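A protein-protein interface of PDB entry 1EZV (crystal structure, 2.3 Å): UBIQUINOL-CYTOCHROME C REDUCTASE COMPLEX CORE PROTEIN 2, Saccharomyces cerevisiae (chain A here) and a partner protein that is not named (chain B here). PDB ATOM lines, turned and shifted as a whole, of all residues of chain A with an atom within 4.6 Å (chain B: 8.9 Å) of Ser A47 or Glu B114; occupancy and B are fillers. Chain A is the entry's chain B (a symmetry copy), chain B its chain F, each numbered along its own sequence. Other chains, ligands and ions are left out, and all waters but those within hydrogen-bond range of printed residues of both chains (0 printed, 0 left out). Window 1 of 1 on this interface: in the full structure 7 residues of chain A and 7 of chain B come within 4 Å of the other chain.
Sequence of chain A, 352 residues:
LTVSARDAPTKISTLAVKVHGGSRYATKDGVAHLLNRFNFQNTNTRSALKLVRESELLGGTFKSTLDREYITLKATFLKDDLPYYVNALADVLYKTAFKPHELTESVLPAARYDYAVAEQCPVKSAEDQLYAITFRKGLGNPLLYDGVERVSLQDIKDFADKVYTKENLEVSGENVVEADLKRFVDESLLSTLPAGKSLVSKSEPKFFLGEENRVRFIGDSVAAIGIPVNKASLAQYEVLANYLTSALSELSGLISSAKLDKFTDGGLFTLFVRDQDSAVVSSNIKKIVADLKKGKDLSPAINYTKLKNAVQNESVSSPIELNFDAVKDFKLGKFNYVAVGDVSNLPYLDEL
The side-chain carboxylate of Glu B114 sits at hydrogen-bond distance from the side-chain hydroxyl of Ser A47, 2.7 Å away.
NZ of Lys B115 lies within salt-bridge range of OD2 of Asp B119, 2.7 Å away.
OG of Ser A47 is in hydrogen-bond range of N of Lys A50 (3.1 Å).
Among the printed residues, merely in contact across the chains: Lys A50 with Glu B114, Leu A49 with Leu B118, Leu A49 with Lys B115 and Lys A50 with Leu B118.
Arg A46 touches none of the printed residues of chain B.
Of chain B, only Glu B114 comes within 4 Å of Ser A47.
Ala A48 touches none of the printed residues of chain B.
Of the printed residues of chain B, Leu A49 touches Lys B115 (3.9 Å) and Leu B118 (3.8 Å).
Of the printed residues of chain B, Lys A50 touches Glu B114 (3.6 Å) and Leu B118 (3.9 Å).
Of chain A, only Ser A47 and Lys A50 come within 4 Å of Glu B114.
Printed residues of chain A within 4 Å of Lys B115: Leu A49.
Printed residues of chain A within 4 Å of Leu B118: Leu A49 and Lys A50.
The nearest residue of chain B that does not touch Ser A47 is Leu B118 (5.5 Å).
The nearest residue of chain A that does not touch Glu B114 is Leu A49 (4.4 Å).
The nearest printed residue of chain B that does not touch Lys A50 is Glu B117 (7.4 Å).
Of the 8 printed residues of chain A, 3 touch a printed residue of chain B.
Along chain A the printed residues that touch a printed residue of chain B span positions 47 to 50.
Of the 15 printed residues of chain B, 3 touch a printed residue of chain A.
Along chain B the printed residues that touch a printed residue of chain A span positions 114 to 118.
Among the printed residues, 5 pairs touch across the chains.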
ATOM      1  N   ASN A  42      34.273  22.567  19.586  1.00  0.00           N
ATOM      2  CA  ASN A  42      33.775  23.910  19.284  1.00  0.00           C
ATOM      3  C   ASN A  42      34.621  24.621  18.234  1.00  0.00           C
ATOM      4  O   ASN A  42      35.852  24.560  18.270  1.00  0.00           O
ATOM      5  CB  ASN A  42      33.717  24.767  20.555  1.00  0.00           C
ATOM      6  CG  ASN A  42      32.524  24.429  21.437  1.00  0.00           C
ATOM      7  OD1 ASN A  42      31.634  23.673  21.046  1.00  0.00           O
ATOM      8  ND2 ASN A  42      32.501  25.001  22.635  1.00  0.00           N
ATOM      9  N   THR A  45      32.409  29.898  15.627  1.00  0.00           N
ATOM     10  CA  THR A  45      31.074  30.367  15.245  1.00  0.00           C
ATOM     11  C   THR A  45      29.972  29.379  15.645  1.00  0.00           C
ATOM     12  O   THR A  45      28.792  29.747  15.724  1.00  0.00           O
ATOM     13  CB  THR A  45      30.970  30.633  13.707  1.00  0.00           C
ATOM     14  OG1 THR A  45      31.049  29.394  12.987  1.00  0.00           O
ATOM     15  CG2 THR A  45      32.089  31.560  13.246  1.00  0.00           C
ATOM     16  N   ARG A  46      30.369  28.128  15.876  1.00  0.00           N
ATOM     17  CA  ARG A  46      29.435  27.021  16.080  1.00  0.00           C
ATOM     18  C   ARG A  46      29.958  26.152  17.216  1.00  0.00           C
ATOM     19  O   ARG A  46      31.118  25.740  17.204  1.00  0.00           O
ATOM     20  CB  ARG A  46      29.343  26.176  14.807  1.00  0.00           C
ATOM     21  CG  ARG A  46      27.971  25.604  14.502  1.00  0.00           C
ATOM     22  CD  ARG A  46      27.444  26.161  13.180  1.00  0.00           C
ATOM     23  NE  ARG A  46      27.461  25.198  12.074  1.00  0.00           N
ATOM     24  CZ  ARG A  46      28.532  24.884  11.345  1.00  0.00           C
ATOM     25  NH1 ARG A  46      28.397  24.094  10.291  1.00  0.00           N
ATOM     26  NH2 ARG A  46      29.746  25.277  11.708  1.00  0.00           N
ATOM     27  N   SER A  47      29.111  25.886  18.204  1.00  0.00           N
ATOM     28  CA  SER A  47      29.460  24.932  19.261  1.00  0.00           C
ATOM     29  C   SER A  47      29.281  23.499  18.767  1.00  0.00           C
ATOM     30  O   SER A  47      28.452  23.231  17.884  1.00  0.00           O
ATOM     31  CB  SER A  47      28.595  25.159  20.505  1.00  0.00           C
ATOM     32  OG  SER A  47      27.251  24.781  20.264  1.00  0.00           O
ATOM     33  N   ALA A  48      30.064  22.587  19.339  1.00  0.00           N
ATOM     34  CA  ALA A  48      29.910  21.155  19.097  1.00  0.00           C
ATOM     35  C   ALA A  48      28.451  20.720  19.236  1.00  0.00           C
ATOM     36  O   ALA A  48      27.933  19.985  18.396  1.00  0.00           O
ATOM     37  CB  ALA A  48      30.794  20.367  20.056  1.00  0.00           C
ATOM     38  N   LEU A  49      27.758  21.278  20.224  1.00  0.00           N
ATOM     39  CA  LEU A  49      26.353  20.951  20.447  1.00  0.00           C
ATOM     40  C   LEU A  49      25.468  21.332  19.254  1.00  0.00           C
ATOM     41  O   LEU A  49      24.721  20.494  18.740  1.00  0.00           O
ATOM     42  CB  LEU A  49      25.850  21.635  21.730  1.00  0.00           C
ATOM     43  CG  LEU A  49      24.343  21.641  21.995  1.00  0.00           C
ATOM     44  CD1 LEU A  49      23.846  20.234  22.273  1.00  0.00           C
ATOM     45  CD2 LEU A  49      24.047  22.552  23.169  1.00  0.00           C
ATOM     46  N   LYS A  50      25.581  22.579  18.798  1.00  0.00           N
ATOM     47  CA  LYS A  50      24.764  23.073  17.683  1.00  0.00           C
ATOM     48  C   LYS A  50      25.051  22.337  16.371  1.00  0.00           C
ATOM     49  O   LYS A  50      24.130  22.031  15.612  1.00  0.00           O
ATOM     50  CB  LYS A  50      24.970  24.580  17.480  1.00  0.00           C
ATOM     51  CG  LYS A  50      24.056  25.167  16.413  1.00  0.00           C
ATOM     52  CD  LYS A  50      23.960  26.674  16.497  1.00  0.00           C
ATOM     53  CE  LYS A  50      22.793  27.179  15.647  1.00  0.00           C
ATOM     54  NZ  LYS A  50      22.645  28.667  15.690  1.00  0.00           N
ATOM     55  N   LEU A  51      26.319  22.006  16.140  1.00  0.00           N
ATOM     56  CA  LEU A  51      26.708  21.245  14.960  1.00  0.00           C
ATOM     57  C   LEU A  51      25.938  19.932  14.880  1.00  0.00           C
ATOM     58  O   LEU A  51      25.317  19.632  13.856  1.00  0.00           O
ATOM     59  CB  LEU A  51      28.208  20.958  14.982  1.00  0.00           C
ATOM     60  CG  LEU A  51      28.753  20.157  13.796  1.00  0.00           C
ATOM     61  CD1 LEU A  51      28.377  20.857  12.487  1.00  0.00           C
ATOM     62  CD2 LEU A  51      30.272  20.031  13.927  1.00  0.00           C
ATOM     63  N   GLU B 107      30.389  32.513  29.954  1.00  0.00           N
ATOM     64  CA  GLU B 107      30.561  31.414  29.013  1.00  0.00           C
ATOM     65  C   GLU B 107      29.603  30.255  29.315  1.00  0.00           C
ATOM     66  O   GLU B 107      28.879  29.797  28.429  1.00  0.00           O
ATOM     67  CB  GLU B 107      32.014  30.937  29.049  1.00  0.00           C
ATOM     68  CG  GLU B 107      32.307  29.760  28.142  1.00  0.00           C
ATOM     69  CD  GLU B 107      33.788  29.411  28.084  1.00  0.00           C
ATOM     70  OE1 GLU B 107      34.224  28.982  26.997  1.00  0.00           O
ATOM     71  OE2 GLU B 107      34.510  29.548  29.110  1.00  0.00           O
ATOM     72  N   ALA B 108      29.528  29.854  30.584  1.00  0.00           N
ATOM     73  CA  ALA B 108      28.615  28.788  31.000  1.00  0.00           C
ATOM     74  C   ALA B 108      27.138  29.151  30.832  1.00  0.00           C
ATOM     75  O   ALA B 108      26.347  28.318  30.421  1.00  0.00           O
ATOM     76  CB  ALA B 108      28.897  28.388  32.438  1.00  0.00           C
ATOM     77  N   GLU B 109      26.769  30.401  31.097  1.00  0.00           N
ATOM     78  CA  GLU B 109      25.379  30.825  30.880  1.00  0.00           C
ATOM     79  C   GLU B 109      24.968  30.768  29.409  1.00  0.00           C
ATOM     80  O   GLU B 109      23.856  30.356  29.081  1.00  0.00           O
ATOM     81  CB  GLU B 109      25.144  32.234  31.424  1.00  0.00           C
ATOM     82  CG  GLU B 109      24.996  32.284  32.940  1.00  0.00           C
ATOM     83  CD  GLU B 109      24.777  33.688  33.475  1.00  0.00           C
ATOM     84  OE1 GLU B 109      25.053  33.911  34.665  1.00  0.00           O
ATOM     85  OE2 GLU B 109      24.314  34.566  32.724  1.00  0.00           O
ATOM     86  N   ALA B 110      25.884  31.143  28.524  1.00  0.00           N
ATOM     87  CA  ALA B 110      25.615  31.117  27.091  1.00  0.00           C
ATOM     88  C   ALA B 110      25.451  29.674  26.617  1.00  0.00           C
ATOM     89  O   ALA B 110      24.467  29.342  25.943  1.00  0.00           O
ATOM     90  CB  ALA B 110      26.752  31.812  26.324  1.00  0.00           C
ATOM     91  N   ALA B 111      26.362  28.801  27.046  1.00  0.00           N
ATOM     92  CA  ALA B 111      26.258  27.380  26.708  1.00  0.00           C
ATOM     93  C   ALA B 111      24.921  26.798  27.170  1.00  0.00           C
ATOM     94  O   ALA B 111      24.212  26.168  26.388  1.00  0.00           O
ATOM     95  CB  ALA B 111      27.406  26.604  27.323  1.00  0.00           C
ATOM     96  N   ALA B 112      24.527  27.137  28.395  1.00  0.00           N
ATOM     97  CA  ALA B 112      23.265  26.678  28.968  1.00  0.00           C
ATOM     98  C   ALA B 112      22.054  27.232  28.220  1.00  0.00           C
ATOM     99  O   ALA B 112      21.101  26.503  27.941  1.00  0.00           O
ATOM    100  CB  ALA B 112      23.193  27.058  30.449  1.00  0.00           C
ATOM    101  N   LYS B 113      22.093  28.522  27.899  1.00  0.00           N
ATOM    102  CA  LYS B 113      21.007  29.161  27.162  1.00  0.00           C
ATOM    103  C   LYS B 113      20.815  28.549  25.768  1.00  0.00           C
ATOM    104  O   LYS B 113      19.687  28.278  25.356  1.00  0.00           O
ATOM    105  CB  LYS B 113      21.266  30.667  27.051  1.00  0.00           C
ATOM    106  CG  LYS B 113      20.140  31.447  26.380  1.00  0.00           C
ATOM    107  CD  LYS B 113      18.791  31.181  27.054  1.00  0.00           C
ATOM    108  CE  LYS B 113      18.324  32.381  27.883  1.00  0.00           C
ATOM    109  NZ  LYS B 113      18.052  33.588  27.045  1.00  0.00           N
ATOM    110  N   GLU B 114      21.918  28.233  25.095  1.00  0.00           N
ATOM    111  CA  GLU B 114      21.846  27.572  23.793  1.00  0.00           C
ATOM    112  C   GLU B 114      21.210  26.177  23.873  1.00  0.00           C
ATOM    113  O   GLU B 114      20.355  25.828  23.046  1.00  0.00           O
ATOM    114  CB  GLU B 114      23.239  27.479  23.159  1.00  0.00           C
ATOM    115  CG  GLU B 114      23.234  26.895  21.752  1.00  0.00           C
ATOM    116  CD  GLU B 114      24.606  26.907  21.098  1.00  0.00           C
ATOM    117  OE1 GLU B 114      25.574  26.405  21.710  1.00  0.00           O
ATOM    118  OE2 GLU B 114      24.711  27.406  19.956  1.00  0.00           O
ATOM    119  N   LYS B 115      21.589  25.398  24.889  1.00  0.00           N
ATOM    120  CA  LYS B 115      21.005  24.073  25.072  1.00  0.00           C
ATOM    121  C   LYS B 115      19.503  24.167  25.287  1.00  0.00           C
ATOM    122  O   LYS B 115      18.729  23.432  24.671  1.00  0.00           O
ATOM    123  CB  LYS B 115      21.641  23.344  26.255  1.00  0.00           C
ATOM    124  CG  LYS B 115      21.205  21.889  26.361  1.00  0.00           C
ATOM    125  CD  LYS B 115      21.461  21.319  27.748  1.00  0.00           C
ATOM    126  CE  LYS B 115      21.266  19.810  27.771  1.00  0.00           C
ATOM    127  NZ  LYS B 115      19.939  19.406  27.227  1.00  0.00           N
ATOM    128  N   ASP B 116      19.090  25.151  26.073  1.00  0.00           N
ATOM    129  CA  ASP B 116      17.677  25.350  26.337  1.00  0.00           C
ATOM    130  C   ASP B 116      16.949  25.762  25.053  1.00  0.00           C
ATOM    131  O   ASP B 116      15.843  25.291  24.777  1.00  0.00           O
ATOM    132  CB  ASP B 116      17.501  26.408  27.430  1.00  0.00           C
ATOM    133  CG  ASP B 116      16.070  26.504  27.925  1.00  0.00           C
ATOM    134  OD1 ASP B 116      15.630  25.587  28.657  1.00  0.00           O
ATOM    135  OD2 ASP B 116      15.380  27.484  27.564  1.00  0.00           O
ATOM    136  N   GLU B 117      17.635  26.542  24.218  1.00  0.00           N
ATOM    137  CA  GLU B 117      17.093  26.982  22.933  1.00  0.00           C
ATOM    138  C   GLU B 117      16.964  25.815  21.963  1.00  0.00           C
ATOM    139  O   GLU B 117      15.900  25.603  21.372  1.00  0.00           O
ATOM    140  CB  GLU B 117      17.989  28.064  22.327  1.00  0.00           C
ATOM    141  CG  GLU B 117      17.353  29.447  22.288  1.00  0.00           C
ATOM    142  CD  GLU B 117      18.339  30.570  22.571  1.00  0.00           C
ATOM    143  OE1 GLU B 117      19.519  30.474  22.155  1.00  0.00           O
ATOM    144  OE2 GLU B 117      17.929  31.556  23.224  1.00  0.00           O
ATOM    145  N   LEU B 118      18.021  25.012  21.871  1.00  0.00           N
ATOM    146  CA  LEU B 118      18.028  23.867  20.971  1.00  0.00           C
ATOM    147  C   LEU B 118      17.108  22.716  21.402  1.00  0.00           C
ATOM    148  O   LEU B 118      16.520  22.051  20.548  1.00  0.00           O
ATOM    149  CB  LEU B 118      19.462  23.367  20.777  1.00  0.00           C
ATOM    150  CG  LEU B 118      20.395  24.365  20.075  1.00  0.00           C
ATOM    151  CD1 LEU B 118      21.828  23.885  20.163  1.00  0.00           C
ATOM    152  CD2 LEU B 118      19.978  24.545  18.619  1.00  0.00           C
ATOM    153  N   ASP B 119      16.935  22.508  22.711  1.00  0.00           N
ATOM    154  CA  ASP B 119      15.996  21.488  23.205  1.00  0.00           C
ATOM    155  C   ASP B 119      14.543  21.865  22.875  1.00  0.00           C
ATOM    156  O   ASP B 119      13.651  21.018  22.900  1.00  0.00           O
ATOM    157  CB  ASP B 119      16.121  21.301  24.730  1.00  0.00           C
ATOM    158  CG  ASP B 119      17.432  20.653  25.151  1.00  0.00           C
ATOM    159  OD1 ASP B 119      18.104  20.018  24.316  1.00  0.00           O
ATOM    160  OD2 ASP B 119      17.786  20.769  26.344  1.00  0.00           O
ATOM    161  N   ASN B 120      14.308  23.138  22.574  1.00  0.00           N
ATOM    162  CA  ASN B 120      12.949  23.615  22.378  1.00  0.00           C
ATOM    163  C   ASN B 120      12.688  24.219  20.998  1.00  0.00           C
ATOM    164  O   ASN B 120      11.631  24.811  20.781  1.00  0.00           O
ATOM    165  CB  ASN B 120      12.589  24.632  23.467  1.00  0.00           C
ATOM    166  CG  ASN B 120      12.519  24.007  24.851  1.00  0.00           C
ATOM    167  OD1 ASN B 120      11.737  23.091  25.091  1.00  0.00           O
ATOM    168  ND2 ASN B 120      13.371  24.475  25.755  1.00  0.00           N
ATOM    169  N   ILE B 121      13.614  24.027  20.056  1.00  0.00           N
ATOM    170  CA  ILE B 121      13.436  24.561  18.700  1.00  0.00           C
ATOM    171  C   ILE B 121      12.202  23.995  18.009  1.00  0.00           C
ATOM    172  O   ILE B 121      11.984  22.788  18.016  1.00  0.00           O
ATOM    173  CB  ILE B 121      14.657  24.282  17.775  1.00  0.00           C
ATOM    174  CG1 ILE B 121      15.119  22.835  17.925  1.00  0.00           C
ATOM    175  CG2 ILE B 121      15.775  25.270  18.061  1.00  0.00           C
ATOM    176  CD1 ILE B 121      16.384  22.517  17.163  1.00  0.00           C
